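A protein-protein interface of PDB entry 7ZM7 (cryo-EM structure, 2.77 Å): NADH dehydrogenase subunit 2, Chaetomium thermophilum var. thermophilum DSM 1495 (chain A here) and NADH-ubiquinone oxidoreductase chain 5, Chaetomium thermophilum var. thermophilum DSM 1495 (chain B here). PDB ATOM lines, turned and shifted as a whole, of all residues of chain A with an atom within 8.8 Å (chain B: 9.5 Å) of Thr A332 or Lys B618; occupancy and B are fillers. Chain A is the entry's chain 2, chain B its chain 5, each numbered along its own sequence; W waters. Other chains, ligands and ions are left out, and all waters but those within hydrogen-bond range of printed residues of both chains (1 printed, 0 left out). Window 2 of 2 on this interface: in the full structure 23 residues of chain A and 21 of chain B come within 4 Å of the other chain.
OG of Ser B617 sits at hydrogen-bond distance from OG1 of Thr A332 (3.0 Å).
The side-chain hydroxyl of Ser B617 is in hydrogen-bond range of the backbone carbonyl oxygen of Leu B613. OG of Ser B621 is in hydrogen-bond range of O of Ser B617 (2.9 Å). OG of Ser B617 sits at hydrogen-bond distance from O of Val B614, at 3.3 Å. The backbone carbonyl oxygen of Lys B618 is in hydrogen-bond range of the side-chain hydroxyl of Ser B621 (3.2 Å). NE2 of Gln A333 is in hydrogen-bond range of O of Val A329, at 3.2 Å.
Among the printed residues, pairs that only touch across the chains: Val A328 with Ser B617, Val A329 with Ile B620, Val A328 with Leu B616, Tyr A342 with Ser B624, Val A329 with Ser B617, Thr A332 with Val B614 and Thr A332 with Lys B618.
Thr A332 touches three residues of chain B. Lys B618 touches just one residue of chain A: Thr A332 (3.97 Å). No residue of chain B comes within 4 Å of Gly A330. No residue of chain B comes within 4 Å of Gln A333. Of chain A, only Val A328, Val A329 and Thr A332 come within 4 Å of Ser B617. No residue of chain A comes within 4 Å of Ser B621. Of the printed residues of chain A, Val B614 touches Thr A332 (3.96 Å). Of the printed residues of chain B, Tyr A342 touches Ser B624 (3.9 Å). Of the printed residues of chain A, Ile B620 touches Val A329. Of the printed residues of chain A, Leu B616 touches Val A328. Of the printed residues of chain B, Val A328 touches Leu B616 (3.8 Å) and Ser B617 (3.2 Å). Arg A335 touches none of the printed residues of chain B. The nearest printed residue of chain A that does not touch Leu B616 is Val A329 (6.5 Å).
Of the 20 printed residues of chain B, 6 touch a printed residue of chain A. Hydrophobic or aromatic side chains of chain B that line the printed part of chain A: Leu B616 and Ile B620. Hydrophobic or aromatic side chains of chain A within 4 Å of the printed part of chain B: Val A328, Val A329 and Tyr A342. Among the printed residues, 8 pairs touch across the chains.
Water W1 lies within hydrogen-bond range of OG of Ser B624 (2.5 Å) and OH of Tyr A342 (2.9 Å).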
ATOM      1  N   GLY A 326     -20.881  27.467  28.259  1.00  0.00           N
ATOM      2  CA  GLY A 326     -21.228  28.706  27.588  1.00  0.00           C
ATOM      3  C   GLY A 326     -20.234  29.820  27.836  1.00  0.00           C
ATOM      4  O   GLY A 326     -20.019  30.671  26.976  1.00  0.00           O
ATOM      5  N   THR A 327     -19.624  29.844  29.016  1.00  0.00           N
ATOM      6  CA  THR A 327     -18.677  30.913  29.290  1.00  0.00           C
ATOM      7  C   THR A 327     -17.247  30.533  28.965  1.00  0.00           C
ATOM      8  O   THR A 327     -16.439  31.417  28.682  1.00  0.00           O
ATOM      9  CB  THR A 327     -18.748  31.372  30.751  1.00  0.00           C
ATOM     10  OG1 THR A 327     -18.231  30.352  31.610  1.00  0.00           O
ATOM     11  CG2 THR A 327     -20.153  31.727  31.151  1.00  0.00           C
ATOM     12  N   VAL A 328     -16.896  29.255  28.997  1.00  0.00           N
ATOM     13  CA  VAL A 328     -15.512  28.902  28.703  1.00  0.00           C
ATOM     14  C   VAL A 328     -15.276  28.861  27.206  1.00  0.00           C
ATOM     15  O   VAL A 328     -14.351  29.499  26.698  1.00  0.00           O
ATOM     16  CB  VAL A 328     -15.122  27.577  29.378  1.00  0.00           C
ATOM     17  CG1 VAL A 328     -13.917  26.976  28.687  1.00  0.00           C
ATOM     18  CG2 VAL A 328     -14.804  27.826  30.831  1.00  0.00           C
ATOM     19  N   VAL A 329     -16.125  28.145  26.469  1.00  0.00           N
ATOM     20  CA  VAL A 329     -15.899  27.998  25.035  1.00  0.00           C
ATOM     21  C   VAL A 329     -16.011  29.319  24.289  1.00  0.00           C
ATOM     22  O   VAL A 329     -15.426  29.465  23.215  1.00  0.00           O
ATOM     23  CB  VAL A 329     -16.855  26.946  24.447  1.00  0.00           C
ATOM     24  CG1 VAL A 329     -16.462  26.612  23.042  1.00  0.00           C
ATOM     25  CG2 VAL A 329     -16.798  25.713  25.278  1.00  0.00           C
ATOM     26  N   GLY A 330     -16.720  30.296  24.830  1.00  0.00           N
ATOM     27  CA  GLY A 330     -16.846  31.559  24.137  1.00  0.00           C
ATOM     28  C   GLY A 330     -15.609  32.419  24.136  1.00  0.00           C
ATOM     29  O   GLY A 330     -15.557  33.400  23.399  1.00  0.00           O
ATOM     30  N   LEU A 331     -14.601  32.055  24.924  1.00  0.00           N
ATOM     31  CA  LEU A 331     -13.403  32.873  25.039  1.00  0.00           C
ATOM     32  C   LEU A 331     -12.651  32.965  23.720  1.00  0.00           C
ATOM     33  O   LEU A 331     -12.086  34.012  23.397  1.00  0.00           O
ATOM     34  CB  LEU A 331     -12.506  32.307  26.135  1.00  0.00           C
ATOM     35  CG  LEU A 331     -13.056  32.447  27.547  1.00  0.00           C
ATOM     36  CD1 LEU A 331     -12.138  31.818  28.563  1.00  0.00           C
ATOM     37  CD2 LEU A 331     -13.249  33.901  27.845  1.00  0.00           C
ATOM     38  N   THR A 332     -12.618  31.881  22.948  1.00  0.00           N
ATOM     39  CA  THR A 332     -11.805  31.821  21.745  1.00  0.00           C
ATOM     40  C   THR A 332     -12.615  31.969  20.461  1.00  0.00           C
ATOM     41  O   THR A 332     -12.124  31.642  19.383  1.00  0.00           O
ATOM     42  CB  THR A 332     -11.001  30.519  21.709  1.00  0.00           C
ATOM     43  OG1 THR A 332     -11.839  29.422  22.091  1.00  0.00           O
ATOM     44  CG2 THR A 332      -9.781  30.600  22.614  1.00  0.00           C
ATOM     45  N   GLN A 333     -13.839  32.442  20.542  1.00  0.00           N
ATOM     46  CA  GLN A 333     -14.598  32.678  19.332  1.00  0.00           C
ATOM     47  C   GLN A 333     -14.153  33.983  18.685  1.00  0.00           C
ATOM     48  O   GLN A 333     -13.877  34.967  19.368  1.00  0.00           O
ATOM     49  CB  GLN A 333     -16.095  32.700  19.644  1.00  0.00           C
ATOM     50  CG  GLN A 333     -16.564  31.469  20.390  1.00  0.00           C
ATOM     51  CD  GLN A 333     -16.372  30.190  19.602  1.00  0.00           C
ATOM     52  OE1 GLN A 333     -17.112  29.916  18.675  1.00  0.00           O
ATOM     53  NE2 GLN A 333     -15.378  29.405  19.974  1.00  0.00           N
ATOM     54  N   PHE A 334     -14.046  33.976  17.362  1.00  0.00           N
ATOM     55  CA  PHE A 334     -13.798  35.195  16.616  1.00  0.00           C
ATOM     56  C   PHE A 334     -14.960  35.581  15.726  1.00  0.00           C
ATOM     57  O   PHE A 334     -14.953  36.676  15.167  1.00  0.00           O
ATOM     58  CB  PHE A 334     -12.509  35.075  15.784  1.00  0.00           C
ATOM     59  CG  PHE A 334     -12.548  34.001  14.754  1.00  0.00           C
ATOM     60  CD1 PHE A 334     -12.225  32.710  15.088  1.00  0.00           C
ATOM     61  CD2 PHE A 334     -12.910  34.278  13.458  1.00  0.00           C
ATOM     62  CE1 PHE A 334     -12.271  31.733  14.168  1.00  0.00           C
ATOM     63  CE2 PHE A 334     -12.955  33.289  12.531  1.00  0.00           C
ATOM     64  CZ  PHE A 334     -12.637  32.016  12.889  1.00  0.00           C
ATOM     65  N   ARG A 335     -15.966  34.736  15.609  1.00  0.00           N
ATOM     66  CA  ARG A 335     -17.153  35.026  14.828  1.00  0.00           C
ATOM     67  C   ARG A 335     -18.265  35.485  15.761  1.00  0.00           C
ATOM     68  O   ARG A 335     -18.556  34.826  16.756  1.00  0.00           O
ATOM     69  CB  ARG A 335     -17.566  33.799  14.022  1.00  0.00           C
ATOM     70  CG  ARG A 335     -16.576  33.487  12.939  1.00  0.00           C
ATOM     71  CD  ARG A 335     -16.913  32.255  12.160  1.00  0.00           C
ATOM     72  NE  ARG A 335     -17.878  32.489  11.096  1.00  0.00           N
ATOM     73  CZ  ARG A 335     -17.671  33.246  10.033  1.00  0.00           C
ATOM     74  NH1 ARG A 335     -18.625  33.376   9.137  1.00  0.00           N
ATOM     75  NH2 ARG A 335     -16.521  33.865   9.856  1.00  0.00           N
ATOM     76  N   ARG A 338     -21.368  33.157  16.338  1.00  0.00           N
ATOM     77  CA  ARG A 338     -20.967  32.052  17.202  1.00  0.00           C
ATOM     78  C   ARG A 338     -20.752  32.525  18.633  1.00  0.00           C
ATOM     79  O   ARG A 338     -21.027  31.790  19.582  1.00  0.00           O
ATOM     80  CB  ARG A 338     -19.691  31.398  16.681  1.00  0.00           C
ATOM     81  CG  ARG A 338     -19.799  30.801  15.325  1.00  0.00           C
ATOM     82  CD  ARG A 338     -18.626  29.928  15.035  1.00  0.00           C
ATOM     83  NE  ARG A 338     -18.511  28.838  15.991  1.00  0.00           N
ATOM     84  CZ  ARG A 338     -19.089  27.654  15.842  1.00  0.00           C
ATOM     85  NH1 ARG A 338     -19.829  27.402  14.767  1.00  0.00           N
ATOM     86  NH2 ARG A 338     -18.925  26.724  16.765  1.00  0.00           N
ATOM     87  N   LEU A 339     -20.226  33.738  18.804  1.00  0.00           N
ATOM     88  CA  LEU A 339     -20.080  34.304  20.136  1.00  0.00           C
ATOM     89  C   LEU A 339     -21.429  34.484  20.803  1.00  0.00           C
ATOM     90  O   LEU A 339     -21.595  34.172  21.984  1.00  0.00           O
ATOM     91  CB  LEU A 339     -19.382  35.655  20.061  1.00  0.00           C
ATOM     92  CG  LEU A 339     -19.152  36.247  21.452  1.00  0.00           C
ATOM     93  CD1 LEU A 339     -18.229  35.345  22.222  1.00  0.00           C
ATOM     94  CD2 LEU A 339     -18.659  37.635  21.448  1.00  0.00           C
ATOM     95  N   TYR A 342     -23.065  31.227  21.972  1.00  0.00           N
ATOM     96  CA  TYR A 342     -22.546  30.720  23.235  1.00  0.00           C
ATOM     97  C   TYR A 342     -22.995  31.569  24.408  1.00  0.00           C
ATOM     98  O   TYR A 342     -23.250  31.043  25.494  1.00  0.00           O
ATOM     99  CB  TYR A 342     -21.028  30.649  23.184  1.00  0.00           C
ATOM    100  CG  TYR A 342     -20.537  29.407  22.509  1.00  0.00           C
ATOM    101  CD1 TYR A 342     -20.721  28.169  23.095  1.00  0.00           C
ATOM    102  CD2 TYR A 342     -19.919  29.462  21.274  1.00  0.00           C
ATOM    103  CE1 TYR A 342     -20.296  27.029  22.479  1.00  0.00           C
ATOM    104  CE2 TYR A 342     -19.494  28.322  20.655  1.00  0.00           C
ATOM    105  CZ  TYR A 342     -19.683  27.116  21.268  1.00  0.00           C
ATOM    106  OH  TYR A 342     -19.264  25.970  20.663  1.00  0.00           O
ATOM    107  N   ILE A 415     -15.714  39.627  14.525  1.00  0.00           N
ATOM    108  CA  ILE A 415     -15.680  40.650  15.552  1.00  0.00           C
ATOM    109  C   ILE A 415     -14.708  41.757  15.171  1.00  0.00           C
ATOM    110  O   ILE A 415     -14.916  42.920  15.517  1.00  0.00           O
ATOM    111  CB  ILE A 415     -15.363  40.002  16.906  1.00  0.00           C
ATOM    112  CG1 ILE A 415     -16.505  39.059  17.281  1.00  0.00           C
ATOM    113  CG2 ILE A 415     -15.148  41.061  17.978  1.00  0.00           C
ATOM    114  CD1 ILE A 415     -16.223  38.121  18.381  1.00  0.00           C
ATOM    115  N   ILE A 476     -15.773  34.731  33.899  1.00  0.00           N
ATOM    116  CA  ILE A 476     -15.191  34.166  32.690  1.00  0.00           C
ATOM    117  C   ILE A 476     -15.962  34.619  31.462  1.00  0.00           C
ATOM    118  O   ILE A 476     -15.373  34.953  30.430  1.00  0.00           O
ATOM    119  CB  ILE A 476     -15.126  32.631  32.790  1.00  0.00           C
ATOM    120  CG1 ILE A 476     -14.284  32.209  33.992  1.00  0.00           C
ATOM    121  CG2 ILE A 476     -14.547  32.032  31.533  1.00  0.00           C
ATOM    122  CD1 ILE A 476     -14.338  30.746  34.272  1.00  0.00           C
ATOM    123  N   VAL A 479     -15.209  38.032  30.027  1.00  0.00           N
ATOM    124  CA  VAL A 479     -13.981  38.236  29.271  1.00  0.00           C
ATOM    125  C   VAL A 479     -14.286  38.380  27.791  1.00  0.00           C
ATOM    126  O   VAL A 479     -13.774  39.280  27.127  1.00  0.00           O
ATOM    127  CB  VAL A 479     -12.984  37.098  29.538  1.00  0.00           C
ATOM    128  CG1 VAL A 479     -11.802  37.222  28.626  1.00  0.00           C
ATOM    129  CG2 VAL A 479     -12.546  37.112  30.972  1.00  0.00           C
ATOM    130  N   TYR A 480     -15.134  37.511  27.251  1.00  0.00           N
ATOM    131  CA  TYR A 480     -15.405  37.601  25.825  1.00  0.00           C
ATOM    132  C   TYR A 480     -16.380  38.715  25.493  1.00  0.00           C
ATOM    133  O   TYR A 480     -16.433  39.143  24.342  1.00  0.00           O
ATOM    134  CB  TYR A 480     -15.880  36.251  25.259  1.00  0.00           C
ATOM    135  CG  TYR A 480     -17.166  35.658  25.790  1.00  0.00           C
ATOM    136  CD1 TYR A 480     -18.397  36.224  25.497  1.00  0.00           C
ATOM    137  CD2 TYR A 480     -17.148  34.496  26.543  1.00  0.00           C
ATOM    138  CE1 TYR A 480     -19.557  35.675  25.959  1.00  0.00           C
ATOM    139  CE2 TYR A 480     -18.306  33.941  27.011  1.00  0.00           C
ATOM    140  CZ  TYR A 480     -19.512  34.531  26.712  1.00  0.00           C
ATOM    141  OH  TYR A 480     -20.671  33.969  27.187  1.00  0.00           O
ATOM    142  N   ASN A 483     -13.995  41.753  25.142  1.00  0.00           N
ATOM    143  CA  ASN A 483     -13.273  41.708  23.878  1.00  0.00           C
ATOM    144  C   ASN A 483     -14.074  42.368  22.764  1.00  0.00           C
ATOM    145  O   ASN A 483     -13.506  43.024  21.890  1.00  0.00           O
ATOM    146  CB  ASN A 483     -12.946  40.262  23.521  1.00  0.00           C
ATOM    147  CG  ASN A 483     -11.817  39.710  24.331  1.00  0.00           C
ATOM    148  OD1 ASN A 483     -11.896  38.605  24.844  1.00  0.00           O
ATOM    149  ND2 ASN A 483     -10.746  40.471  24.448  1.00  0.00           N
ATOM    150  N   GLU B 610      -5.427  32.783  32.431  1.00  0.00           N
ATOM    151  CA  GLU B 610      -5.476  33.103  31.010  1.00  0.00           C
ATOM    152  C   GLU B 610      -4.902  31.975  30.167  1.00  0.00           C
ATOM    153  O   GLU B 610      -5.527  31.523  29.205  1.00  0.00           O
ATOM    154  CB  GLU B 610      -4.701  34.383  30.745  1.00  0.00           C
ATOM    155  CG  GLU B 610      -4.759  34.829  29.320  1.00  0.00           C
ATOM    156  CD  GLU B 610      -4.023  36.114  29.098  1.00  0.00           C
ATOM    157  OE1 GLU B 610      -3.455  36.634  30.068  1.00  0.00           O
ATOM    158  OE2 GLU B 610      -4.004  36.608  27.960  1.00  0.00           O
ATOM    159  N   ARG B 611      -3.707  31.503  30.521  1.00  0.00           N
ATOM    160  CA  ARG B 611      -3.046  30.496  29.706  1.00  0.00           C
ATOM    161  C   ARG B 611      -3.810  29.184  29.728  1.00  0.00           C
ATOM    162  O   ARG B 611      -3.961  28.533  28.690  1.00  0.00           O
ATOM    163  CB  ARG B 611      -1.616  30.286  30.186  1.00  0.00           C
ATOM    164  CG  ARG B 611      -0.657  31.270  29.630  1.00  0.00           C
ATOM    165  CD  ARG B 611       0.481  31.461  30.568  1.00  0.00           C
ATOM    166  NE  ARG B 611       0.936  30.180  31.084  1.00  0.00           N
ATOM    167  CZ  ARG B 611       2.043  29.565  30.684  1.00  0.00           C
ATOM    168  NH1 ARG B 611       2.383  28.405  31.216  1.00  0.00           N
ATOM    169  NH2 ARG B 611       2.798  30.099  29.737  1.00  0.00           N
ATOM    170  N   GLY B 612      -4.303  28.787  30.897  1.00  0.00           N
ATOM    171  CA  GLY B 612      -5.038  27.538  30.991  1.00  0.00           C
ATOM    172  C   GLY B 612      -6.375  27.573  30.278  1.00  0.00           C
ATOM    173  O   GLY B 612      -6.709  26.656  29.526  1.00  0.00           O
ATOM    174  N   LEU B 613      -7.155  28.628  30.496  1.00  0.00           N
ATOM    175  CA  LEU B 613      -8.510  28.658  29.968  1.00  0.00           C
ATOM    176  C   LEU B 613      -8.518  28.726  28.446  1.00  0.00           C
ATOM    177  O   LEU B 613      -9.337  28.069  27.798  1.00  0.00           O
ATOM    178  CB  LEU B 613      -9.275  29.828  30.583  1.00  0.00           C
ATOM    179  CG  LEU B 613      -9.737  29.626  32.027  1.00  0.00           C
ATOM    180  CD1 LEU B 613     -10.489  30.812  32.501  1.00  0.00           C
ATOM    181  CD2 LEU B 613     -10.573  28.375  32.176  1.00  0.00           C
ATOM    182  N   VAL B 614      -7.615  29.509  27.857  1.00  0.00           N
ATOM    183  CA  VAL B 614      -7.562  29.624  26.403  1.00  0.00           C
ATOM    184  C   VAL B 614      -7.234  28.282  25.774  1.00  0.00           C
ATOM    185  O   VAL B 614      -7.774  27.921  24.723  1.00  0.00           O
ATOM    186  CB  VAL B 614      -6.545  30.701  25.995  1.00  0.00           C
ATOM    187  CG1 VAL B 614      -6.157  30.545  24.543  1.00  0.00           C
ATOM    188  CG2 VAL B 614      -7.107  32.066  26.248  1.00  0.00           C
ATOM    189  N   LYS B 615      -6.319  27.536  26.385  1.00  0.00           N
ATOM    190  CA  LYS B 615      -6.033  26.196  25.909  1.00  0.00           C
ATOM    191  C   LYS B 615      -7.231  25.278  26.113  1.00  0.00           C
ATOM    192  O   LYS B 615      -7.570  24.487  25.229  1.00  0.00           O
ATOM    193  CB  LYS B 615      -4.796  25.655  26.615  1.00  0.00           C
ATOM    194  CG  LYS B 615      -4.265  24.372  26.033  1.00  0.00           C
ATOM    195  CD  LYS B 615      -3.003  23.910  26.749  1.00  0.00           C
ATOM    196  CE  LYS B 615      -1.815  24.807  26.443  1.00  0.00           C
ATOM    197  NZ  LYS B 615      -1.550  24.898  24.983  1.00  0.00           N
ATOM    198  N   LEU B 616      -7.885  25.379  27.267  1.00  0.00           N
ATOM    199  CA  LEU B 616      -9.076  24.585  27.529  1.00  0.00           C
ATOM    200  C   LEU B 616     -10.125  24.790  26.448  1.00  0.00           C
ATOM    201  O   LEU B 616     -10.652  23.823  25.895  1.00  0.00           O
ATOM    202  CB  LEU B 616      -9.645  24.963  28.893  1.00  0.00           C
ATOM    203  CG  LEU B 616     -10.914  24.303  29.428  1.00  0.00           C
ATOM    204  CD1 LEU B 616     -10.697  22.866  29.682  1.00  0.00           C
ATOM    205  CD2 LEU B 616     -11.422  24.991  30.665  1.00  0.00           C
ATOM    206  N   SER B 617     -10.425  26.047  26.122  1.00  0.00           N
ATOM    207  CA  SER B 617     -11.526  26.333  25.215  1.00  0.00           C
ATOM    208  C   SER B 617     -11.173  26.034  23.768  1.00  0.00           C
ATOM    209  O   SER B 617     -12.065  25.728  22.972  1.00  0.00           O
ATOM    210  CB  SER B 617     -11.979  27.778  25.372  1.00  0.00           C
ATOM    211  OG  SER B 617     -11.025  28.694  24.894  1.00  0.00           O
ATOM    212  N   LYS B 618      -9.898  26.119  23.400  1.00  0.00           N
ATOM    213  CA  LYS B 618      -9.495  25.693  22.067  1.00  0.00           C
ATOM    214  C   LYS B 618      -9.736  24.205  21.873  1.00  0.00           C
ATOM    215  O   LYS B 618     -10.120  23.764  20.788  1.00  0.00           O
ATOM    216  CB  LYS B 618      -8.027  26.028  21.829  1.00  0.00           C
ATOM    217  CG  LYS B 618      -7.784  27.417  21.348  1.00  0.00           C
ATOM    218  CD  LYS B 618      -6.379  27.558  20.854  1.00  0.00           C
ATOM    219  CE  LYS B 618      -5.415  27.392  22.003  1.00  0.00           C
ATOM    220  NZ  LYS B 618      -4.078  27.942  21.716  1.00  0.00           N
ATOM    221  N   ASN B 619      -9.489  23.416  22.910  1.00  0.00           N
ATOM    222  CA  ASN B 619      -9.732  21.986  22.839  1.00  0.00           C
ATOM    223  C   ASN B 619     -11.217  21.670  22.743  1.00  0.00           C
ATOM    224  O   ASN B 619     -11.626  20.854  21.912  1.00  0.00           O
ATOM    225  CB  ASN B 619      -9.119  21.309  24.054  1.00  0.00           C
ATOM    226  CG  ASN B 619      -7.605  21.354  24.043  1.00  0.00           C
ATOM    227  OD1 ASN B 619      -6.967  20.896  23.103  1.00  0.00           O
ATOM    228  ND2 ASN B 619      -7.024  21.918  25.087  1.00  0.00           N
ATOM    229  N   ILE B 620     -12.043  22.297  23.578  1.00  0.00           N
ATOM    230  CA  ILE B 620     -13.474  22.026  23.534  1.00  0.00           C
ATOM    231  C   ILE B 620     -14.052  22.435  22.186  1.00  0.00           C
ATOM    232  O   ILE B 620     -14.889  21.734  21.616  1.00  0.00           O
ATOM    233  CB  ILE B 620     -14.194  22.734  24.694  1.00  0.00           C
ATOM    234  CG1 ILE B 620     -13.551  22.379  26.027  1.00  0.00           C
ATOM    235  CG2 ILE B 620     -15.639  22.336  24.729  1.00  0.00           C
ATOM    236  CD1 ILE B 620     -14.107  23.128  27.196  1.00  0.00           C
ATOM    237  N   SER B 621     -13.640  23.586  21.665  1.00  0.00           N
ATOM    238  CA  SER B 621     -14.129  23.986  20.359  1.00  0.00           C
ATOM    239  C   SER B 621     -13.513  23.176  19.229  1.00  0.00           C
ATOM    240  O   SER B 621     -13.982  23.281  18.097  1.00  0.00           O
ATOM    241  CB  SER B 621     -13.901  25.479  20.148  1.00  0.00           C
ATOM    242  OG  SER B 621     -12.535  25.804  20.149  1.00  0.00           O
ATOM    243  N   SER B 622     -12.494  22.366  19.505  1.00  0.00           N
ATOM    244  CA  SER B 622     -12.030  21.385  18.532  1.00  0.00           C
ATOM    245  C   SER B 622     -12.978  20.208  18.405  1.00  0.00           C
ATOM    246  O   SER B 622     -12.799  19.382  17.508  1.00  0.00           O
ATOM    247  CB  SER B 622     -10.643  20.870  18.908  1.00  0.00           C
ATOM    248  OG  SER B 622     -10.693  19.998  20.025  1.00  0.00           O
ATOM    249  N   LEU B 623     -13.951  20.093  19.298  1.00  0.00           N
ATOM    250  CA  LEU B 623     -15.000  19.096  19.175  1.00  0.00           C
ATOM    251  C   LEU B 623     -16.044  19.477  18.137  1.00  0.00           C
ATOM    252  O   LEU B 623     -16.654  18.593  17.533  1.00  0.00           O
ATOM    253  CB  LEU B 623     -15.666  18.891  20.533  1.00  0.00           C
ATOM    254  CG  LEU B 623     -14.844  18.099  21.540  1.00  0.00           C
ATOM    255  CD1 LEU B 623     -15.315  18.368  22.952  1.00  0.00           C
ATOM    256  CD2 LEU B 623     -14.949  16.630  21.225  1.00  0.00           C
ATOM    257  N   SER B 624     -16.266  20.767  17.920  1.00  0.00           N
ATOM    258  CA  SER B 624     -17.400  21.255  17.136  1.00  0.00           C
ATOM    259  C   SER B 624     -17.038  21.260  15.658  1.00  0.00           C
ATOM    260  O   SER B 624     -16.394  22.185  15.171  1.00  0.00           O
ATOM    261  CB  SER B 624     -17.802  22.645  17.608  1.00  0.00           C
ATOM    262  OG  SER B 624     -18.364  22.588  18.904  1.00  0.00           O
ATOM    263  N   LEU B 665      -8.658  17.061  31.085  1.00  0.00           N
ATOM    264  CA  LEU B 665      -8.231  16.423  29.845  1.00  0.00           C
ATOM    265  C   LEU B 665      -8.313  17.381  28.662  1.00  0.00           C
ATOM    266  O   LEU B 665      -7.518  17.271  27.726  1.00  0.00           O
ATOM    267  CB  LEU B 665      -9.071  15.178  29.586  1.00  0.00           C
ATOM    268  CG  LEU B 665      -9.025  14.087  30.654  1.00  0.00           C
ATOM    269  CD1 LEU B 665      -9.859  12.903  30.215  1.00  0.00           C
ATOM    270  CD2 LEU B 665      -7.613  13.665  30.989  1.00  0.00           C
ATOM    271  N   MET B 666      -9.261  18.314  28.676  1.00  0.00           N
ATOM    272  CA  MET B 666      -9.280  19.397  27.705  1.00  0.00           C
ATOM    273  C   MET B 666      -8.173  20.415  27.931  1.00  0.00           C
ATOM    274  O   MET B 666      -7.794  21.106  26.983  1.00  0.00           O
ATOM    275  CB  MET B 666     -10.631  20.115  27.735  1.00  0.00           C
ATOM    276  CG  MET B 666     -11.846  19.315  27.299  1.00  0.00           C
ATOM    277  SD  MET B 666     -11.756  18.756  25.587  1.00  0.00           S
ATOM    278  CE  MET B 666     -11.305  17.038  25.821  1.00  0.00           C
ATOM    279  N   MET B 667      -7.659  20.552  29.157  1.00  0.00           N
ATOM    280  CA  MET B 667      -6.471  21.371  29.356  1.00  0.00           C
ATOM    281  C   MET B 667      -5.259  20.747  28.688  1.00  0.00           C
ATOM    282  O   MET B 667      -4.388  21.467  28.186  1.00  0.00           O
ATOM    283  CB  MET B 667      -6.192  21.572  30.844  1.00  0.00           C
ATOM    284  CG  MET B 667      -7.176  22.456  31.576  1.00  0.00           C
ATOM    285  SD  MET B 667      -6.734  24.198  31.481  1.00  0.00           S
ATOM    286  CE  MET B 667      -7.481  24.836  32.981  1.00  0.00           C
ATOM    287  N   ILE B 668      -5.176  19.423  28.677  1.00  0.00           N
ATOM    288  CA  ILE B 668      -4.045  18.740  28.061  1.00  0.00           C
ATOM    289  C   ILE B 668      -4.294  18.616  26.565  1.00  0.00           C
ATOM    290  O   ILE B 668      -5.381  18.215  26.135  1.00  0.00           O
ATOM    291  CB  ILE B 668      -3.823  17.365  28.705  1.00  0.00           C
ATOM    292  CG1 ILE B 668      -3.492  17.529  30.186  1.00  0.00           C
ATOM    293  CG2 ILE B 668      -2.710  16.618  27.991  1.00  0.00           C
ATOM    294  CD1 ILE B 668      -3.514  16.236  30.955  1.00  0.00           C
ATOM    295  N   GLY B 669      -3.288  18.978  25.767  1.00  0.00           N
ATOM    296  CA  GLY B 669      -3.379  18.872  24.328  1.00  0.00           C
ATOM    297  C   GLY B 669      -2.878  17.536  23.810  1.00  0.00           C
ATOM    298  O   GLY B 669      -2.388  16.687  24.551  1.00  0.00           O
HETATM  299  O   HOH W   1     -18.124  23.348  21.282  1.00  0.00           O
